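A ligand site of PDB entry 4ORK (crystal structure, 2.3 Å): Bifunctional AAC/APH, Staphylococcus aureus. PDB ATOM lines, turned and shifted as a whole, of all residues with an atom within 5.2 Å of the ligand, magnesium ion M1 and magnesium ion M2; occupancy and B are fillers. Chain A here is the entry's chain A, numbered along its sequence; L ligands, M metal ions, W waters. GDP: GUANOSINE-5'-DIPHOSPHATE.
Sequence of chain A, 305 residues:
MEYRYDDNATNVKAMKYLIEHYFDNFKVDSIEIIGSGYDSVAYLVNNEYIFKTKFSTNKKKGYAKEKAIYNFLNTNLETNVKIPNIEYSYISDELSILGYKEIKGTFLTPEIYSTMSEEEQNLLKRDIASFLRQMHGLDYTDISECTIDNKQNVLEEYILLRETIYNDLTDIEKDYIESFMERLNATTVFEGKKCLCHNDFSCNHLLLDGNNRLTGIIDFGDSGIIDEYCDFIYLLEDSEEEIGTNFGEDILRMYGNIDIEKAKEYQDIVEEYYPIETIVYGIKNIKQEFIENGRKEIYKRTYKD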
ATOM      1  N   ILE A  34     -14.800  20.856 -19.411  1.00  0.00           N
ATOM      2  CA  ILE A  34     -14.537  21.464 -18.122  1.00  0.00           C
ATOM      3  C   ILE A  34     -15.094  20.654 -16.969  1.00  0.00           C
ATOM      4  O   ILE A  34     -14.914  21.028 -15.806  1.00  0.00           O
ATOM      5  CB  ILE A  34     -15.101  22.896 -18.022  1.00  0.00           C
ATOM      6  CG1 ILE A  34     -16.606  22.900 -18.226  1.00  0.00           C
ATOM      7  CG2 ILE A  34     -14.427  23.784 -19.030  1.00  0.00           C
ATOM      8  CD1 ILE A  34     -17.383  23.096 -16.967  1.00  0.00           C
ATOM      9  N   GLY A  35     -15.776  19.569 -17.274  1.00  0.00           N
ATOM     10  CA  GLY A  35     -16.330  18.750 -16.206  1.00  0.00           C
ATOM     11  C   GLY A  35     -17.148  17.579 -16.681  1.00  0.00           C
ATOM     12  O   GLY A  35     -17.541  17.501 -17.843  1.00  0.00           O
ATOM     13  N   SER A  36     -17.402  16.681 -15.749  1.00  0.00           N
ATOM     14  CA  SER A  36     -18.123  15.452 -16.057  1.00  0.00           C
ATOM     15  C   SER A  36     -18.567  14.812 -14.762  1.00  0.00           C
ATOM     16  O   SER A  36     -17.765  14.598 -13.851  1.00  0.00           O
ATOM     17  CB  SER A  36     -17.234  14.495 -16.864  1.00  0.00           C
ATOM     18  OG  SER A  36     -17.859  13.232 -17.051  1.00  0.00           O
ATOM     19  N   GLY A  37     -19.859  14.560 -14.669  1.00  0.00           N
ATOM     20  CA  GLY A  37     -20.414  13.779 -13.574  1.00  0.00           C
ATOM     21  C   GLY A  37     -20.689  12.395 -14.118  1.00  0.00           C
ATOM     22  O   GLY A  37     -20.151  11.986 -15.164  1.00  0.00           O
ATOM     23  N   TYR A  38     -21.541  11.654 -13.414  1.00  0.00           N
ATOM     24  CA  TYR A  38     -21.888  10.311 -13.856  1.00  0.00           C
ATOM     25  C   TYR A  38     -22.996  10.320 -14.903  1.00  0.00           C
ATOM     26  O   TYR A  38     -23.370   9.273 -15.436  1.00  0.00           O
ATOM     27  CB  TYR A  38     -22.297   9.463 -12.644  1.00  0.00           C
ATOM     28  CG  TYR A  38     -21.119   8.977 -11.835  1.00  0.00           C
ATOM     29  CD1 TYR A  38     -20.359   7.887 -12.279  1.00  0.00           C
ATOM     30  CD2 TYR A  38     -20.760   9.579 -10.638  1.00  0.00           C
ATOM     31  CE1 TYR A  38     -19.279   7.421 -11.549  1.00  0.00           C
ATOM     32  CE2 TYR A  38     -19.671   9.125  -9.891  1.00  0.00           C
ATOM     33  CZ  TYR A  38     -18.939   8.038 -10.357  1.00  0.00           C
ATOM     34  OH  TYR A  38     -17.857   7.572  -9.652  1.00  0.00           O
ATOM     35  N   ASP A  39     -23.492  11.522 -15.215  1.00  0.00           N
ATOM     36  CA  ASP A  39     -24.587  11.700 -16.172  1.00  0.00           C
ATOM     37  C   ASP A  39     -24.204  12.467 -17.432  1.00  0.00           C
ATOM     38  O   ASP A  39     -24.569  12.085 -18.541  1.00  0.00           O
ATOM     39  CB  ASP A  39     -25.771  12.395 -15.502  1.00  0.00           C
ATOM     40  CG  ASP A  39     -26.502  11.498 -14.522  1.00  0.00           C
ATOM     41  OD1 ASP A  39     -27.199  10.576 -14.999  1.00  0.00           O
ATOM     42  OD2 ASP A  39     -26.386  11.707 -13.297  1.00  0.00           O
ATOM     43  N   SER A  40     -23.462  13.560 -17.263  1.00  0.00           N
ATOM     44  CA  SER A  40     -23.206  14.465 -18.363  1.00  0.00           C
ATOM     45  C   SER A  40     -21.731  14.816 -18.537  1.00  0.00           C
ATOM     46  O   SER A  40     -20.914  14.589 -17.637  1.00  0.00           O
ATOM     47  CB  SER A  40     -24.003  15.763 -18.171  1.00  0.00           C
ATOM     48  OG  SER A  40     -25.374  15.546 -18.456  1.00  0.00           O
ATOM     49  N   ALA A  42     -19.571  18.324 -19.521  1.00  0.00           N
ATOM     50  CA  ALA A  42     -19.823  19.762 -19.534  1.00  0.00           C
ATOM     51  C   ALA A  42     -18.744  20.542 -20.283  1.00  0.00           C
ATOM     52  O   ALA A  42     -17.556  20.404 -20.025  1.00  0.00           O
ATOM     53  CB  ALA A  42     -19.942  20.276 -18.122  1.00  0.00           C
ATOM     54  N   ILE A  50     -21.899  27.300 -20.699  1.00  0.00           N
ATOM     55  CA  ILE A  50     -21.796  25.871 -20.442  1.00  0.00           C
ATOM     56  C   ILE A  50     -22.773  25.133 -21.337  1.00  0.00           C
ATOM     57  O   ILE A  50     -23.974  25.419 -21.325  1.00  0.00           O
ATOM     58  CB  ILE A  50     -22.075  25.510 -18.985  1.00  0.00           C
ATOM     59  CG1 ILE A  50     -21.128  26.245 -18.034  1.00  0.00           C
ATOM     60  CG2 ILE A  50     -21.977  24.000 -18.812  1.00  0.00           C
ATOM     61  CD1 ILE A  50     -19.718  25.710 -17.999  1.00  0.00           C
ATOM     62  N   LYS A  52     -23.881  21.292 -21.571  1.00  0.00           N
ATOM     63  CA  LYS A  52     -23.748  19.913 -21.124  1.00  0.00           C
ATOM     64  C   LYS A  52     -24.594  18.962 -21.990  1.00  0.00           C
ATOM     65  O   LYS A  52     -25.591  19.375 -22.603  1.00  0.00           O
ATOM     66  CB  LYS A  52     -24.116  19.787 -19.634  1.00  0.00           C
ATOM     67  CG  LYS A  52     -25.538  20.170 -19.302  1.00  0.00           C
ATOM     68  CD  LYS A  52     -25.779  20.322 -17.765  1.00  0.00           C
ATOM     69  CE  LYS A  52     -26.027  18.977 -17.129  1.00  0.00           C
ATOM     70  NZ  LYS A  52     -26.591  19.118 -15.771  1.00  0.00           N
ATOM     71  N   GLU A  66     -35.175  18.767 -16.332  1.00  0.00           N
ATOM     72  CA  GLU A  66     -34.148  19.674 -15.819  1.00  0.00           C
ATOM     73  C   GLU A  66     -34.409  21.077 -16.343  1.00  0.00           C
ATOM     74  O   GLU A  66     -34.365  22.049 -15.591  1.00  0.00           O
ATOM     75  CB  GLU A  66     -32.734  19.235 -16.232  1.00  0.00           C
ATOM     76  CG  GLU A  66     -31.603  19.969 -15.463  1.00  0.00           C
ATOM     77  CD  GLU A  66     -30.181  19.512 -15.826  1.00  0.00           C
ATOM     78  OE1 GLU A  66     -29.246  20.338 -15.745  1.00  0.00           O
ATOM     79  OE2 GLU A  66     -29.979  18.324 -16.177  1.00  0.00           O
ATOM     80  N   TYR A 100     -26.235  27.309 -21.251  1.00  0.00           N
ATOM     81  CA  TYR A 100     -26.501  28.409 -20.332  1.00  0.00           C
ATOM     82  C   TYR A 100     -25.207  29.113 -19.945  1.00  0.00           C
ATOM     83  O   TYR A 100     -24.152  28.497 -19.913  1.00  0.00           O
ATOM     84  CB  TYR A 100     -27.202  27.900 -19.076  1.00  0.00           C
ATOM     85  CG  TYR A 100     -26.479  26.812 -18.328  1.00  0.00           C
ATOM     86  CD1 TYR A 100     -25.558  27.127 -17.332  1.00  0.00           C
ATOM     87  CD2 TYR A 100     -26.712  25.474 -18.608  1.00  0.00           C
ATOM     88  CE1 TYR A 100     -24.892  26.142 -16.643  1.00  0.00           C
ATOM     89  CE2 TYR A 100     -26.047  24.482 -17.931  1.00  0.00           C
ATOM     90  CZ  TYR A 100     -25.138  24.816 -16.936  1.00  0.00           C
ATOM     91  OH  TYR A 100     -24.472  23.831 -16.247  1.00  0.00           O
ATOM     92  N   LYS A 101     -25.302  30.420 -19.700  1.00  0.00           N
ATOM     93  CA  LYS A 101     -24.120  31.166 -19.255  1.00  0.00           C
ATOM     94  C   LYS A 101     -23.519  30.529 -18.018  1.00  0.00           C
ATOM     95  O   LYS A 101     -24.238  30.146 -17.094  1.00  0.00           O
ATOM     96  CB  LYS A 101     -24.461  32.637 -18.972  1.00  0.00           C
ATOM     97  CG  LYS A 101     -24.337  33.507 -20.213  1.00  0.00           C
ATOM     98  CD  LYS A 101     -25.097  34.814 -20.073  1.00  0.00           C
ATOM     99  CE  LYS A 101     -25.253  35.446 -21.459  1.00  0.00           C
ATOM    100  NZ  LYS A 101     -23.997  35.235 -22.235  1.00  0.00           N
ATOM    101  N   GLU A 102     -22.210  30.347 -18.055  1.00  0.00           N
ATOM    102  CA  GLU A 102     -21.454  29.767 -16.961  1.00  0.00           C
ATOM    103  C   GLU A 102     -21.792  30.427 -15.627  1.00  0.00           C
ATOM    104  O   GLU A 102     -21.778  31.656 -15.508  1.00  0.00           O
ATOM    105  CB  GLU A 102     -19.952  29.920 -17.240  1.00  0.00           C
ATOM    106  CG  GLU A 102     -19.034  29.281 -16.225  1.00  0.00           C
ATOM    107  CD  GLU A 102     -17.589  29.680 -16.423  1.00  0.00           C
ATOM    108  OE1 GLU A 102     -17.335  30.790 -16.951  1.00  0.00           O
ATOM    109  OE2 GLU A 102     -16.708  28.894 -16.025  1.00  0.00           O
ATOM    110  N   ILE A 103     -22.118  29.616 -14.620  1.00  0.00           N
ATOM    111  CA  ILE A 103     -22.161  30.109 -13.248  1.00  0.00           C
ATOM    112  C   ILE A 103     -20.732  30.291 -12.754  1.00  0.00           C
ATOM    113  O   ILE A 103     -20.033  29.308 -12.530  1.00  0.00           O
ATOM    114  CB  ILE A 103     -22.910  29.173 -12.308  1.00  0.00           C
ATOM    115  CG1 ILE A 103     -24.252  28.801 -12.926  1.00  0.00           C
ATOM    116  CG2 ILE A 103     -23.117  29.838 -10.954  1.00  0.00           C
ATOM    117  CD1 ILE A 103     -25.139  29.988 -13.094  1.00  0.00           C
ATOM    118  N   LYS A 104     -20.313  31.538 -12.604  1.00  0.00           N
ATOM    119  CA  LYS A 104     -18.913  31.813 -12.274  1.00  0.00           C
ATOM    120  C   LYS A 104     -18.697  31.791 -10.768  1.00  0.00           C
ATOM    121  O   LYS A 104     -19.571  32.171  -9.994  1.00  0.00           O
ATOM    122  CB  LYS A 104     -18.467  33.146 -12.874  1.00  0.00           C
ATOM    123  CG  LYS A 104     -18.246  33.084 -14.385  1.00  0.00           C
ATOM    124  CD  LYS A 104     -17.559  34.338 -14.882  1.00  0.00           C
ATOM    125  CE  LYS A 104     -17.668  34.486 -16.393  1.00  0.00           C
ATOM    126  NZ  LYS A 104     -17.251  33.272 -17.153  1.00  0.00           N
ATOM    127  N   GLY A 105     -17.536  31.303 -10.356  1.00  0.00           N
ATOM    128  CA  GLY A 105     -17.236  31.137  -8.952  1.00  0.00           C
ATOM    129  C   GLY A 105     -16.272  29.990  -8.711  1.00  0.00           C
ATOM    130  O   GLY A 105     -15.849  29.315  -9.656  1.00  0.00           O
ATOM    131  N   PHE A 107     -15.591  26.363  -6.685  1.00  0.00           N
ATOM    132  CA  PHE A 107     -16.300  25.253  -6.078  1.00  0.00           C
ATOM    133  C   PHE A 107     -15.874  25.019  -4.636  1.00  0.00           C
ATOM    134  O   PHE A 107     -14.695  24.968  -4.319  1.00  0.00           O
ATOM    135  CB  PHE A 107     -16.134  23.979  -6.909  1.00  0.00           C
ATOM    136  CG  PHE A 107     -17.004  23.953  -8.101  1.00  0.00           C
ATOM    137  CD1 PHE A 107     -18.376  23.933  -7.940  1.00  0.00           C
ATOM    138  CD2 PHE A 107     -16.474  24.020  -9.376  1.00  0.00           C
ATOM    139  CE1 PHE A 107     -19.221  23.959  -9.050  1.00  0.00           C
ATOM    140  CE2 PHE A 107     -17.310  24.035 -10.490  1.00  0.00           C
ATOM    141  CZ  PHE A 107     -18.680  24.007 -10.325  1.00  0.00           C
ATOM    142  N   ASP A 200     -29.247  16.560  -5.582  1.00  0.00           N
ATOM    143  CA  ASP A 200     -27.876  16.106  -5.727  1.00  0.00           C
ATOM    144  C   ASP A 200     -26.983  17.115  -5.048  1.00  0.00           C
ATOM    145  O   ASP A 200     -25.967  17.557  -5.596  1.00  0.00           O
ATOM    146  CB  ASP A 200     -27.504  15.907  -7.189  1.00  0.00           C
ATOM    147  CG  ASP A 200     -26.297  14.994  -7.370  1.00  0.00           C
ATOM    148  OD1 ASP A 200     -25.844  14.381  -6.355  1.00  0.00           O
ATOM    149  OD2 ASP A 200     -25.794  14.913  -8.508  1.00  0.00           O
ATOM    150  N   ASN A 204     -19.668  19.785  -4.590  1.00  0.00           N
ATOM    151  CA  ASN A 204     -19.140  20.003  -5.935  1.00  0.00           C
ATOM    152  C   ASN A 204     -20.110  20.737  -6.849  1.00  0.00           C
ATOM    153  O   ASN A 204     -19.733  21.183  -7.933  1.00  0.00           O
ATOM    154  CB  ASN A 204     -18.729  18.663  -6.549  1.00  0.00           C
ATOM    155  CG  ASN A 204     -19.903  17.727  -6.780  1.00  0.00           C
ATOM    156  OD1 ASN A 204     -20.788  17.600  -5.937  1.00  0.00           O
ATOM    157  ND2 ASN A 204     -19.912  17.065  -7.926  1.00  0.00           N
ATOM    158  N   HIS A 205     -21.349  20.902  -6.394  1.00  0.00           N
ATOM    159  CA  HIS A 205     -22.286  21.745  -7.120  1.00  0.00           C
ATOM    160  C   HIS A 205     -22.406  23.182  -6.545  1.00  0.00           C
ATOM    161  O   HIS A 205     -23.168  24.007  -7.056  1.00  0.00           O
ATOM    162  CB  HIS A 205     -23.663  21.102  -7.137  1.00  0.00           C
ATOM    163  CG  HIS A 205     -23.693  19.809  -7.905  1.00  0.00           C
ATOM    164  ND1 HIS A 205     -24.514  18.769  -7.544  1.00  0.00           N
ATOM    165  CD2 HIS A 205     -22.977  19.380  -8.965  1.00  0.00           C
ATOM    166  CE1 HIS A 205     -24.315  17.754  -8.371  1.00  0.00           C
ATOM    167  NE2 HIS A 205     -23.397  18.103  -9.237  1.00  0.00           N
ATOM    168  N   LEU A 207     -21.140  26.885  -5.754  1.00  0.00           N
ATOM    169  CA  LEU A 207     -20.118  27.874  -6.089  1.00  0.00           C
ATOM    170  C   LEU A 207     -20.015  29.021  -5.084  1.00  0.00           C
ATOM    171  O   LEU A 207     -21.024  29.479  -4.550  1.00  0.00           O
ATOM    172  CB  LEU A 207     -20.386  28.434  -7.477  1.00  0.00           C
ATOM    173  CG  LEU A 207     -20.075  27.355  -8.496  1.00  0.00           C
ATOM    174  CD1 LEU A 207     -21.062  27.410  -9.619  1.00  0.00           C
ATOM    175  CD2 LEU A 207     -18.645  27.519  -9.000  1.00  0.00           C
ATOM    176  N   ILE A 218     -25.240  24.633  -9.263  1.00  0.00           N
ATOM    177  CA  ILE A 218     -25.372  23.978 -10.544  1.00  0.00           C
ATOM    178  C   ILE A 218     -26.004  22.591 -10.380  1.00  0.00           C
ATOM    179  O   ILE A 218     -26.224  22.079  -9.247  1.00  0.00           O
ATOM    180  CB  ILE A 218     -24.011  23.835 -11.233  1.00  0.00           C
ATOM    181  CG1 ILE A 218     -23.095  22.978 -10.364  1.00  0.00           C
ATOM    182  CG2 ILE A 218     -23.351  25.212 -11.502  1.00  0.00           C
ATOM    183  CD1 ILE A 218     -21.825  22.605 -11.033  1.00  0.00           C
ATOM    184  N   ASP A 219     -26.326  21.997 -11.538  1.00  0.00           N
ATOM    185  CA  ASP A 219     -26.761  20.620 -11.678  1.00  0.00           C
ATOM    186  C   ASP A 219     -28.025  20.277 -10.947  1.00  0.00           C
ATOM    187  O   ASP A 219     -28.012  19.492  -9.986  1.00  0.00           O
ATOM    188  CB  ASP A 219     -25.678  19.656 -11.206  1.00  0.00           C
ATOM    189  CG  ASP A 219     -25.903  18.202 -11.691  1.00  0.00           C
ATOM    190  OD1 ASP A 219     -27.013  17.852 -12.166  1.00  0.00           O
ATOM    191  OD2 ASP A 219     -24.964  17.409 -11.543  1.00  0.00           O
ATOM    192  N   GLY A 221     -30.017  18.529 -12.356  1.00  0.00           N
ATOM    193  CA  GLY A 221     -30.312  17.400 -13.229  1.00  0.00           C
ATOM    194  C   GLY A 221     -31.122  16.266 -12.628  1.00  0.00           C
ATOM    195  O   GLY A 221     -31.748  15.506 -13.354  1.00  0.00           O
ATOM    196  N   ASP A 222     -31.133  16.161 -11.297  1.00  0.00           N
ATOM    197  CA  ASP A 222     -31.924  15.126 -10.631  1.00  0.00           C
ATOM    198  C   ASP A 222     -33.064  15.716  -9.809  1.00  0.00           C
ATOM    199  O   ASP A 222     -33.661  15.002  -9.009  1.00  0.00           O
ATOM    200  CB  ASP A 222     -31.057  14.279  -9.712  1.00  0.00           C
ATOM    201  CG  ASP A 222     -29.924  13.618 -10.443  1.00  0.00           C
ATOM    202  OD1 ASP A 222     -29.945  13.614 -11.692  1.00  0.00           O
ATOM    203  OD2 ASP A 222     -29.028  13.076  -9.768  1.00  0.00           O
HETATM  204  PB  GDP L   1     -23.806  15.763 -13.921  1.00  0.00           P
HETATM  205  O1B GDP L   1     -25.257  15.614 -13.644  1.00  0.00           O
HETATM  206  O2B GDP L   1     -23.063  15.647 -12.607  1.00  0.00           O
HETATM  207  O3B GDP L   1     -23.287  14.617 -14.726  1.00  0.00           O
HETATM  208  O3A GDP L   1     -23.588  17.149 -14.707  1.00  0.00           O
HETATM  209  PA  GDP L   1     -23.394  18.600 -13.962  1.00  0.00           P
HETATM  210  O1A GDP L   1     -23.167  18.386 -12.470  1.00  0.00           O
HETATM  211  O2A GDP L   1     -24.466  19.628 -14.251  1.00  0.00           O
HETATM  212  O5' GDP L   1     -22.073  19.194 -14.655  1.00  0.00           O
HETATM  213  C5' GDP L   1     -20.870  18.426 -14.622  1.00  0.00           C
HETATM  214  C4' GDP L   1     -19.774  19.375 -14.184  1.00  0.00           C
HETATM  215  O4' GDP L   1     -19.634  20.496 -15.045  1.00  0.00           O
HETATM  216  C3' GDP L   1     -20.093  19.992 -12.810  1.00  0.00           C
HETATM  217  O3' GDP L   1     -19.709  19.125 -11.764  1.00  0.00           O
HETATM  218  C2' GDP L   1     -19.208  21.205 -12.812  1.00  0.00           C
HETATM  219  O2' GDP L   1     -17.911  20.704 -12.576  1.00  0.00           O
HETATM  220  C1' GDP L   1     -19.256  21.647 -14.270  1.00  0.00           C
HETATM  221  N9  GDP L   1     -20.207  22.782 -14.497  1.00  0.00           N
HETATM  222  C8  GDP L   1     -21.445  22.704 -15.001  1.00  0.00           C
HETATM  223  N7  GDP L   1     -22.034  23.934 -15.070  1.00  0.00           N
HETATM  224  C5  GDP L   1     -21.156  24.827 -14.602  1.00  0.00           C
HETATM  225  C6  GDP L   1     -21.130  26.293 -14.399  1.00  0.00           C
HETATM  226  O6  GDP L   1     -22.101  27.021 -14.695  1.00  0.00           O
HETATM  227  N1  GDP L   1     -20.009  26.820 -13.863  1.00  0.00           N
HETATM  228  C2  GDP L   1     -18.945  26.065 -13.540  1.00  0.00           C
HETATM  229  N2  GDP L   1     -17.852  26.678 -13.024  1.00  0.00           N
HETATM  230  N3  GDP L   1     -18.897  24.723 -13.709  1.00  0.00           N
HETATM  231  C4  GDP L   1     -19.950  24.067 -14.222  1.00  0.00           C
HETATM  232 MG    MG M   1     -22.934  16.876 -11.103  1.00  0.00          MG
HETATM  233 MG    MG M   2     -26.565  15.605 -12.023  1.00  0.00          MG
HETATM  234  O   HOH W   1     -25.967  13.651 -11.527  1.00  0.00           O
HETATM  235  O   HOH W   2     -27.372  15.602 -10.410  1.00  0.00           O
HETATM  236  O   HOH W   3     -23.487  15.425 -10.012  1.00  0.00           O
HETATM  237  O   HOH W   4     -21.045  16.708 -11.179  1.00  0.00           O
HETATM  238  O   HOH W   5     -15.817  26.059 -15.576  1.00  0.00           O
HETATM  239  O   HOH W   6     -28.066  14.906 -13.146  1.00  0.00           O
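The backbone NH of Asp 39 lies within hydrogen-bond range of an oxygen (O3B) of the ligand, at 3.1 Å. N1 of the ligand sits at hydrogen-bond distance from O of Ile 103 (2.8 Å). NZ of Lys 52 lies within salt-bridge range of O2A of the ligand (2.7 Å). N of Gly 37 lies close to O3B of the ligand (3.4 Å). An oxygen (O6) of the ligand lies within hydrogen-bond range of the backbone NH (N) of Ile 103. OH of Tyr 100 is in hydrogen-bond range of N7 of the ligand. O3B of the ligand is in hydrogen-bond range of N of Ser 40 (2.8 Å).
The backbone carbonyl oxygen (O) of Asp 200 is in hydrogen-bond range of a ring nitrogen (ND1) of His 205 (2.7 Å). The side-chain hydroxyl (OG) of Ser 36 lies close to the backbone carbonyl oxygen (O) of Ser 40 (3.4 Å). The backbone NH of Ala 42 lies within hydrogen-bond range of the backbone carbonyl oxygen of Gly 35. OD1 of Asp 219 lies close to NZ of Lys 52 (3.8 Å). The backbone NH of Ile 34 is in hydrogen-bond range of the backbone carbonyl oxygen of Ala 42 (2.9 Å). N of Gly 221 lies close to OD1 of Asp 219, at 3.1 Å. The side-chain amino group of Lys 52 lies within salt-bridge range of the side-chain carboxylate of Glu 66 (2.9 Å). O of His 205 is in hydrogen-bond range of N of Ile 218, 3.1 Å away.
Ile 34 touches the ligand (CD1 to C1', 3.6 Å). CA of Gly 35 touches O4' of the ligand (3.9 Å). Ser 36 touches the ligand. Tyr 38 touches the ligand. Ala 42 touches the ligand (CB to O4', 3.1 Å). Ile 50 touches the ligand. Glu 102 touches the ligand (C to O6, 3.5 Å). CZ of Phe 107 touches N3 of the ligand, 3.5 Å away. CD1 of Ile 218 touches C2' of the ligand, 3.5 Å away. Hydrophobic or aromatic side chains within 4 Å of the ligand: Ile 34, Ala 42, Ile 50, Tyr 100, Ile 103, Phe 107, His 205 and Ile 218. Within 4 Å of the ligand: Ile 34, Gly 35, Ser 36, Gly 37, Tyr 38, Asp 39, Ser 40, Ala 42, Ile 50, Lys 52, Tyr 100, Glu 102, Ile 103, Phe 107, His 205, Ile 218 and Asp 219.
Of the 26 residues printed, 2 come within 4 Å of magnesium ion M1.
Asp 200 touches magnesium ion M2 (OD2 to MG, 3.7 Å). Asp 222 touches magnesium ion M2. Three residues have an atom within 4 Å of magnesium ion M2: Asp 200, Asp 219 and Asp 222.
Magnesium ion M1 is bound by water W3, water W4, an oxygen (O2B) of the ligand, an oxygen (O1A) of the ligand, the side-chain carboxylate of Asp 219 and a ring nitrogen (NE2) of His 205.
Magnesium ion M2 is bound by water W2 (1.8 Å), water W6 (2.0 Å), an oxygen (O1B) of the ligand (2.1 Å), water W1 (2.1 Å), the side-chain carboxylate (OD1) of Asp 219 (2.3 Å) and the side-chain carboxylate (OD2) of Asp 219 (2.5 Å). Magnesium ion M2 has six donor atoms within binding distance.
Water W4 bridges O3' of the ligand and ND2 of Asn 204. Water W2 bridges the side-chain carboxylate (OD2) of Asp 200 (2.6 Å) and the side-chain carboxylate (OD2) of Asp 222 (3.1 Å). Water W1 bridges OD2 of Asp 39 (2.7 Å) and OD2 of Asp 200 (3.3 Å). Water W5 bridges OE2 of Glu 102 (3.0 Å) and N2 of the ligand (3.3 Å).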
